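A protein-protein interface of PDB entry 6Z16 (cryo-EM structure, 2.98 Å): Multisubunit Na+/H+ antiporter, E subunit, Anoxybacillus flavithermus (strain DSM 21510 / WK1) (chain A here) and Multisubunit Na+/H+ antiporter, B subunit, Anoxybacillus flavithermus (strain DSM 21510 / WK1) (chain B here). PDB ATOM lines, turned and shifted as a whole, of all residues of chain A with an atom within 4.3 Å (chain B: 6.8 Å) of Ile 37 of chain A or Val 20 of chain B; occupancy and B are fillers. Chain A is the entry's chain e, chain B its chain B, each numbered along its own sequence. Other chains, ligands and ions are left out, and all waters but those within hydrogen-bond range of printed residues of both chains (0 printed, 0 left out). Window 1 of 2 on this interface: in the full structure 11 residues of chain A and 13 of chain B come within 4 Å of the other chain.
The backbone carbonyl oxygen (O) of Val 20 of chain B lies within hydrogen-bond range of the side-chain hydroxyl (OG) of Ser 23 of chain B, 2.8 Å away.
Among the printed residues, merely in contact across the chains: Ile 33 of chain A with Val 24 of chain B (3.8 Å), Ile 37 of chain A with Pro 17 of chain B (3.8 Å), Ile 37 of chain A with Val 20 of chain B (3.7 Å), Ile 37 of chain A with Leu 21 of chain B (3.6 Å) and Leu 41 of chain A with Pro 17 of chain B (3.8 Å).
Of chain B, only Pro 17, Val 20 and Leu 21 come within 4 Å of Ile 37 of chain A. Printed residues of chain B within 4 Å of Leu 41 of chain A: Pro 17 (3.8 Å). Val 20 of chain B touches just one residue of chain A: Ile 37. Printed residues of chain A within 4 Å of Leu 21 of chain B: Ile 37. Met 43 of chain B touches none of the printed residues of chain A. Thr 44 of chain B touches none of the printed residues of chain A. The nearest printed residue of chain A that does not touch Val 20 of chain B is Ile 40 of chain A (5.0 Å). The nearest printed residue of chain B that does not touch Leu 41 of chain A is Thr 16 of chain B (4.8 Å).
Of the 17 printed residues of chain B, 4 touch a printed residue of chain A. Of the 9 printed residues of chain A, 3 touch a printed residue of chain B. Hydrophobic or aromatic side chains of chain A that line the printed part of chain B: Ile 33, Ile 37 and Leu 41. Among the printed residues, no Asp or Glu carboxylate lies within 4 Å of a Lys or Arg side-chain nitrogen of the other chain.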
ATOM      1  N   ILE A  33     -17.782 -25.801 -15.096  1.00  0.00           N
ATOM      2  CA  ILE A  33     -18.946 -26.350 -14.397  1.00  0.00           C
ATOM      3  C   ILE A  33     -18.680 -26.445 -12.897  1.00  0.00           C
ATOM      4  O   ILE A  33     -19.522 -26.054 -12.077  1.00  0.00           O
ATOM      5  CB  ILE A  33     -19.329 -27.714 -14.999  1.00  0.00           C
ATOM      6  CG1 ILE A  33     -19.799 -27.553 -16.439  1.00  0.00           C
ATOM      7  CG2 ILE A  33     -20.436 -28.371 -14.216  1.00  0.00           C
ATOM      8  CD1 ILE A  33     -19.915 -28.852 -17.169  1.00  0.00           C
ATOM      9  N   GLY A  34     -17.488 -26.909 -12.518  1.00  0.00           N
ATOM     10  CA  GLY A  34     -17.138 -26.974 -11.113  1.00  0.00           C
ATOM     11  C   GLY A  34     -16.964 -25.618 -10.468  1.00  0.00           C
ATOM     12  O   GLY A  34     -17.219 -25.467  -9.272  1.00  0.00           O
ATOM     13  N   LEU A  35     -16.545 -24.614 -11.244  1.00  0.00           N
ATOM     14  CA  LEU A  35     -16.485 -23.249 -10.731  1.00  0.00           C
ATOM     15  C   LEU A  35     -17.874 -22.739 -10.378  1.00  0.00           C
ATOM     16  O   LEU A  35     -18.072 -22.128  -9.317  1.00  0.00           O
ATOM     17  CB  LEU A  35     -15.818 -22.337 -11.763  1.00  0.00           C
ATOM     18  CG  LEU A  35     -15.647 -20.858 -11.421  1.00  0.00           C
ATOM     19  CD1 LEU A  35     -14.772 -20.680 -10.207  1.00  0.00           C
ATOM     20  CD2 LEU A  35     -15.070 -20.115 -12.607  1.00  0.00           C
ATOM     21  N   PHE A  36     -18.859 -23.040 -11.232  1.00  0.00           N
ATOM     22  CA  PHE A  36     -20.241 -22.655 -10.935  1.00  0.00           C
ATOM     23  C   PHE A  36     -20.777 -23.395  -9.710  1.00  0.00           C
ATOM     24  O   PHE A  36     -21.450 -22.797  -8.855  1.00  0.00           O
ATOM     25  CB  PHE A  36     -21.134 -22.921 -12.148  1.00  0.00           C
ATOM     26  CG  PHE A  36     -20.858 -22.022 -13.328  1.00  0.00           C
ATOM     27  CD1 PHE A  36     -20.126 -20.849 -13.184  1.00  0.00           C
ATOM     28  CD2 PHE A  36     -21.334 -22.356 -14.586  1.00  0.00           C
ATOM     29  CE1 PHE A  36     -19.871 -20.037 -14.270  1.00  0.00           C
ATOM     30  CE2 PHE A  36     -21.086 -21.543 -15.677  1.00  0.00           C
ATOM     31  CZ  PHE A  36     -20.354 -20.383 -15.515  1.00  0.00           C
ATOM     32  N   ILE A  37     -20.449 -24.686  -9.596  1.00  0.00           N
ATOM     33  CA  ILE A  37     -20.930 -25.504  -8.484  1.00  0.00           C
ATOM     34  C   ILE A  37     -20.329 -25.047  -7.157  1.00  0.00           C
ATOM     35  O   ILE A  37     -21.037 -24.943  -6.149  1.00  0.00           O
ATOM     36  CB  ILE A  37     -20.638 -26.985  -8.779  1.00  0.00           C
ATOM     37  CG1 ILE A  37     -21.512 -27.436  -9.933  1.00  0.00           C
ATOM     38  CG2 ILE A  37     -20.911 -27.863  -7.587  1.00  0.00           C
ATOM     39  CD1 ILE A  37     -21.086 -28.703 -10.520  1.00  0.00           C
ATOM     40  N   LEU A  38     -19.030 -24.742  -7.135  1.00  0.00           N
ATOM     41  CA  LEU A  38     -18.432 -24.164  -5.938  1.00  0.00           C
ATOM     42  C   LEU A  38     -18.924 -22.756  -5.650  1.00  0.00           C
ATOM     43  O   LEU A  38     -18.866 -22.329  -4.493  1.00  0.00           O
ATOM     44  CB  LEU A  38     -16.911 -24.135  -6.031  1.00  0.00           C
ATOM     45  CG  LEU A  38     -16.103 -25.314  -5.501  1.00  0.00           C
ATOM     46  CD1 LEU A  38     -16.204 -26.520  -6.380  1.00  0.00           C
ATOM     47  CD2 LEU A  38     -14.678 -24.885  -5.383  1.00  0.00           C
ATOM     48  N   PHE A  39     -19.386 -22.014  -6.662  1.00  0.00           N
ATOM     49  CA  PHE A  39     -20.043 -20.749  -6.349  1.00  0.00           C
ATOM     50  C   PHE A  39     -21.387 -20.972  -5.670  1.00  0.00           C
ATOM     51  O   PHE A  39     -21.804 -20.148  -4.847  1.00  0.00           O
ATOM     52  CB  PHE A  39     -20.222 -19.891  -7.601  1.00  0.00           C
ATOM     53  CG  PHE A  39     -20.884 -18.575  -7.322  1.00  0.00           C
ATOM     54  CD1 PHE A  39     -20.205 -17.585  -6.630  1.00  0.00           C
ATOM     55  CD2 PHE A  39     -22.187 -18.333  -7.724  1.00  0.00           C
ATOM     56  CE1 PHE A  39     -20.808 -16.379  -6.346  1.00  0.00           C
ATOM     57  CE2 PHE A  39     -22.796 -17.126  -7.445  1.00  0.00           C
ATOM     58  CZ  PHE A  39     -22.103 -16.149  -6.757  1.00  0.00           C
ATOM     59  N   ILE A  40     -22.079 -22.066  -5.999  1.00  0.00           N
ATOM     60  CA  ILE A  40     -23.332 -22.369  -5.308  1.00  0.00           C
ATOM     61  C   ILE A  40     -23.071 -22.716  -3.845  1.00  0.00           C
ATOM     62  O   ILE A  40     -23.802 -22.280  -2.948  1.00  0.00           O
ATOM     63  CB  ILE A  40     -24.080 -23.496  -6.044  1.00  0.00           C
ATOM     64  CG1 ILE A  40     -24.433 -23.053  -7.461  1.00  0.00           C
ATOM     65  CG2 ILE A  40     -25.349 -23.882  -5.320  1.00  0.00           C
ATOM     66  CD1 ILE A  40     -24.949 -24.168  -8.337  1.00  0.00           C
ATOM     67  N   LEU A  41     -21.988 -23.439  -3.573  1.00  0.00           N
ATOM     68  CA  LEU A  41     -21.710 -24.005  -2.255  1.00  0.00           C
ATOM     69  C   LEU A  41     -20.714 -23.177  -1.453  1.00  0.00           C
ATOM     70  O   LEU A  41     -19.875 -23.733  -0.747  1.00  0.00           O
ATOM     71  CB  LEU A  41     -21.213 -25.438  -2.406  1.00  0.00           C
ATOM     72  CG  LEU A  41     -22.235 -26.400  -3.015  1.00  0.00           C
ATOM     73  CD1 LEU A  41     -21.613 -27.752  -3.297  1.00  0.00           C
ATOM     74  CD2 LEU A  41     -23.434 -26.543  -2.097  1.00  0.00           C
ATOM     75  N   VAL B  15     -23.873 -34.201  -2.054  1.00  0.00           N
ATOM     76  CA  VAL B  15     -24.786 -34.837  -2.999  1.00  0.00           C
ATOM     77  C   VAL B  15     -25.222 -33.863  -4.096  1.00  0.00           C
ATOM     78  O   VAL B  15     -25.409 -34.266  -5.252  1.00  0.00           O
ATOM     79  CB  VAL B  15     -25.964 -35.465  -2.213  1.00  0.00           C
ATOM     80  CG1 VAL B  15     -27.216 -35.592  -3.020  1.00  0.00           C
ATOM     81  CG2 VAL B  15     -25.577 -36.875  -1.794  1.00  0.00           C
ATOM     82  N   THR B  16     -25.312 -32.571  -3.765  1.00  0.00           N
ATOM     83  CA  THR B  16     -25.681 -31.558  -4.758  1.00  0.00           C
ATOM     84  C   THR B  16     -24.751 -31.451  -5.984  1.00  0.00           C
ATOM     85  O   THR B  16     -25.292 -31.324  -7.102  1.00  0.00           O
ATOM     86  CB  THR B  16     -25.838 -30.210  -4.031  1.00  0.00           C
ATOM     87  OG1 THR B  16     -26.814 -30.341  -2.989  1.00  0.00           O
ATOM     88  CG2 THR B  16     -26.286 -29.120  -4.974  1.00  0.00           C
ATOM     89  N   PRO B  17     -23.402 -31.527  -5.885  1.00  0.00           N
ATOM     90  CA  PRO B  17     -22.597 -31.492  -7.122  1.00  0.00           C
ATOM     91  C   PRO B  17     -22.829 -32.640  -8.085  1.00  0.00           C
ATOM     92  O   PRO B  17     -22.771 -32.413  -9.297  1.00  0.00           O
ATOM     93  CB  PRO B  17     -21.155 -31.507  -6.601  1.00  0.00           C
ATOM     94  CG  PRO B  17     -21.234 -30.915  -5.305  1.00  0.00           C
ATOM     95  CD  PRO B  17     -22.505 -31.384  -4.719  1.00  0.00           C
ATOM     96  N   ILE B  18     -23.122 -33.848  -7.612  1.00  0.00           N
ATOM     97  CA  ILE B  18     -23.309 -34.916  -8.589  1.00  0.00           C
ATOM     98  C   ILE B  18     -24.686 -34.815  -9.249  1.00  0.00           C
ATOM     99  O   ILE B  18     -24.841 -35.186 -10.418  1.00  0.00           O
ATOM    100  CB  ILE B  18     -23.031 -36.297  -7.957  1.00  0.00           C
ATOM    101  CG1 ILE B  18     -22.903 -37.361  -9.045  1.00  0.00           C
ATOM    102  CG2 ILE B  18     -24.096 -36.707  -6.971  1.00  0.00           C
ATOM    103  CD1 ILE B  18     -21.810 -37.070 -10.032  1.00  0.00           C
ATOM    104  N   ILE B  19     -25.671 -34.221  -8.564  1.00  0.00           N
ATOM    105  CA  ILE B  19     -26.950 -33.930  -9.205  1.00  0.00           C
ATOM    106  C   ILE B  19     -26.776 -32.860 -10.275  1.00  0.00           C
ATOM    107  O   ILE B  19     -27.347 -32.962 -11.369  1.00  0.00           O
ATOM    108  CB  ILE B  19     -28.001 -33.504  -8.163  1.00  0.00           C
ATOM    109  CG1 ILE B  19     -28.200 -34.581  -7.108  1.00  0.00           C
ATOM    110  CG2 ILE B  19     -29.341 -33.260  -8.825  1.00  0.00           C
ATOM    111  CD1 ILE B  19     -29.083 -34.137  -5.979  1.00  0.00           C
ATOM    112  N   VAL B  20     -25.961 -31.837  -9.995  1.00  0.00           N
ATOM    113  CA  VAL B  20     -25.764 -30.768 -10.972  1.00  0.00           C
ATOM    114  C   VAL B  20     -24.982 -31.270 -12.186  1.00  0.00           C
ATOM    115  O   VAL B  20     -25.342 -30.959 -13.331  1.00  0.00           O
ATOM    116  CB  VAL B  20     -25.096 -29.551 -10.307  1.00  0.00           C
ATOM    117  CG1 VAL B  20     -24.778 -28.488 -11.328  1.00  0.00           C
ATOM    118  CG2 VAL B  20     -26.017 -28.963  -9.266  1.00  0.00           C
ATOM    119  N   LEU B  21     -23.932 -32.078 -11.966  1.00  0.00           N
ATOM    120  CA  LEU B  21     -23.223 -32.698 -13.089  1.00  0.00           C
ATOM    121  C   LEU B  21     -24.126 -33.625 -13.886  1.00  0.00           C
ATOM    122  O   LEU B  21     -24.023 -33.683 -15.114  1.00  0.00           O
ATOM    123  CB  LEU B  21     -21.995 -33.491 -12.636  1.00  0.00           C
ATOM    124  CG  LEU B  21     -20.579 -32.913 -12.587  1.00  0.00           C
ATOM    125  CD1 LEU B  21     -20.278 -32.151 -11.342  1.00  0.00           C
ATOM    126  CD2 LEU B  21     -19.570 -34.018 -12.767  1.00  0.00           C
ATOM    127  N   PHE B  22     -25.023 -34.346 -13.209  1.00  0.00           N
ATOM    128  CA  PHE B  22     -25.928 -35.237 -13.920  1.00  0.00           C
ATOM    129  C   PHE B  22     -26.923 -34.460 -14.773  1.00  0.00           C
ATOM    130  O   PHE B  22     -27.212 -34.859 -15.905  1.00  0.00           O
ATOM    131  CB  PHE B  22     -26.640 -36.149 -12.923  1.00  0.00           C
ATOM    132  CG  PHE B  22     -27.606 -37.099 -13.556  1.00  0.00           C
ATOM    133  CD1 PHE B  22     -27.160 -38.061 -14.446  1.00  0.00           C
ATOM    134  CD2 PHE B  22     -28.946 -37.070 -13.220  1.00  0.00           C
ATOM    135  CE1 PHE B  22     -28.041 -38.948 -15.024  1.00  0.00           C
ATOM    136  CE2 PHE B  22     -29.831 -37.958 -13.790  1.00  0.00           C
ATOM    137  CZ  PHE B  22     -29.378 -38.900 -14.692  1.00  0.00           C
ATOM    138  N   SER B  23     -27.415 -33.326 -14.271  1.00  0.00           N
ATOM    139  CA  SER B  23     -28.364 -32.534 -15.049  1.00  0.00           C
ATOM    140  C   SER B  23     -27.690 -31.866 -16.242  1.00  0.00           C
ATOM    141  O   SER B  23     -28.263 -31.821 -17.338  1.00  0.00           O
ATOM    142  CB  SER B  23     -29.029 -31.494 -14.158  1.00  0.00           C
ATOM    143  OG  SER B  23     -28.093 -30.528 -13.732  1.00  0.00           O
ATOM    144  N   VAL B  24     -26.462 -31.371 -16.062  1.00  0.00           N
ATOM    145  CA  VAL B  24     -25.738 -30.758 -17.174  1.00  0.00           C
ATOM    146  C   VAL B  24     -25.353 -31.808 -18.214  1.00  0.00           C
ATOM    147  O   VAL B  24     -25.407 -31.553 -19.423  1.00  0.00           O
ATOM    148  CB  VAL B  24     -24.521 -29.983 -16.635  1.00  0.00           C
ATOM    149  CG1 VAL B  24     -23.628 -29.485 -17.741  1.00  0.00           C
ATOM    150  CG2 VAL B  24     -24.993 -28.801 -15.816  1.00  0.00           C
ATOM    151  N   GLN B  25     -25.013 -33.020 -17.769  1.00  0.00           N
ATOM    152  CA  GLN B  25     -24.712 -34.095 -18.707  1.00  0.00           C
ATOM    153  C   GLN B  25     -25.956 -34.566 -19.451  1.00  0.00           C
ATOM    154  O   GLN B  25     -25.868 -34.921 -20.633  1.00  0.00           O
ATOM    155  CB  GLN B  25     -24.047 -35.250 -17.962  1.00  0.00           C
ATOM    156  CG  GLN B  25     -23.660 -36.427 -18.834  1.00  0.00           C
ATOM    157  CD  GLN B  25     -22.670 -36.048 -19.910  1.00  0.00           C
ATOM    158  OE1 GLN B  25     -21.744 -35.273 -19.674  1.00  0.00           O
ATOM    159  NE2 GLN B  25     -22.860 -36.590 -21.106  1.00  0.00           N
ATOM    160  N   LEU B  26     -27.118 -34.570 -18.787  1.00  0.00           N
ATOM    161  CA  LEU B  26     -28.376 -34.826 -19.482  1.00  0.00           C
ATOM    162  C   LEU B  26     -28.663 -33.756 -20.522  1.00  0.00           C
ATOM    163  O   LEU B  26     -29.178 -34.055 -21.605  1.00  0.00           O
ATOM    164  CB  LEU B  26     -29.534 -34.900 -18.489  1.00  0.00           C
ATOM    165  CG  LEU B  26     -29.712 -36.145 -17.633  1.00  0.00           C
ATOM    166  CD1 LEU B  26     -30.802 -35.905 -16.614  1.00  0.00           C
ATOM    167  CD2 LEU B  26     -30.056 -37.317 -18.530  1.00  0.00           C
ATOM    168  N   MET B  43     -34.004 -31.552 -13.298  1.00  0.00           N
ATOM    169  CA  MET B  43     -33.112 -32.006 -12.239  1.00  0.00           C
ATOM    170  C   MET B  43     -32.166 -30.932 -11.720  1.00  0.00           C
ATOM    171  O   MET B  43     -31.709 -31.046 -10.575  1.00  0.00           O
ATOM    172  CB  MET B  43     -32.324 -33.242 -12.667  1.00  0.00           C
ATOM    173  CG  MET B  43     -33.234 -34.431 -12.911  1.00  0.00           C
ATOM    174  SD  MET B  43     -34.590 -34.559 -11.710  1.00  0.00           S
ATOM    175  CE  MET B  43     -33.825 -34.873 -10.119  1.00  0.00           C
ATOM    176  N   THR B  44     -31.879 -29.887 -12.500  1.00  0.00           N
ATOM    177  CA  THR B  44     -31.246 -28.708 -11.916  1.00  0.00           C
ATOM    178  C   THR B  44     -32.157 -28.081 -10.870  1.00  0.00           C
ATOM    179  O   THR B  44     -31.713 -27.722  -9.763  1.00  0.00           O
ATOM    180  CB  THR B  44     -30.912 -27.701 -13.011  1.00  0.00           C
ATOM    181  OG1 THR B  44     -30.038 -28.309 -13.966  1.00  0.00           O
ATOM    182  CG2 THR B  44     -30.228 -26.482 -12.425  1.00  0.00           C
ATOM    183  N   ALA B  47     -31.920 -30.246  -7.757  1.00  0.00           N
ATOM    184  CA  ALA B  47     -30.774 -29.907  -6.914  1.00  0.00           C
ATOM    185  C   ALA B  47     -31.059 -28.672  -6.069  1.00  0.00           C
ATOM    186  O   ALA B  47     -30.733 -28.632  -4.870  1.00  0.00           O
ATOM    187  CB  ALA B  47     -29.536 -29.681  -7.775  1.00  0.00           C
ATOM    188  N   ILE B  48     -31.701 -27.665  -6.667  1.00  0.00           N
ATOM    189  CA  ILE B  48     -32.053 -26.482  -5.881  1.00  0.00           C
ATOM    190  C   ILE B  48     -33.156 -26.811  -4.866  1.00  0.00           C
ATOM    191  O   ILE B  48     -33.202 -26.226  -3.778  1.00  0.00           O
ATOM    192  CB  ILE B  48     -32.437 -25.323  -6.818  1.00  0.00           C
ATOM    193  CG1 ILE B  48     -31.326 -25.082  -7.832  1.00  0.00           C
ATOM    194  CG2 ILE B  48     -32.578 -24.028  -6.051  1.00  0.00           C
ATOM    195  CD1 ILE B  48     -31.729 -24.170  -8.956  1.00  0.00           C
ATOM    196  N   TYR B 122     -34.343 -25.254 -21.259  1.00  0.00           N
ATOM    197  CA  TYR B 122     -33.692 -25.492 -19.974  1.00  0.00           C
ATOM    198  C   TYR B 122     -33.968 -24.366 -18.986  1.00  0.00           C
ATOM    199  O   TYR B 122     -34.376 -24.616 -17.842  1.00  0.00           O
ATOM    200  CB  TYR B 122     -32.188 -25.645 -20.207  1.00  0.00           C
ATOM    201  CG  TYR B 122     -31.359 -25.962 -18.988  1.00  0.00           C
ATOM    202  CD1 TYR B 122     -31.217 -27.265 -18.541  1.00  0.00           C
ATOM    203  CD2 TYR B 122     -30.727 -24.951 -18.276  1.00  0.00           C
ATOM    204  CE1 TYR B 122     -30.460 -27.552 -17.426  1.00  0.00           C
ATOM    205  CE2 TYR B 122     -29.983 -25.226 -17.156  1.00  0.00           C
ATOM    206  CZ  TYR B 122     -29.852 -26.525 -16.737  1.00  0.00           C
ATOM    207  OH  TYR B 122     -29.097 -26.799 -15.624  1.00  0.00           O
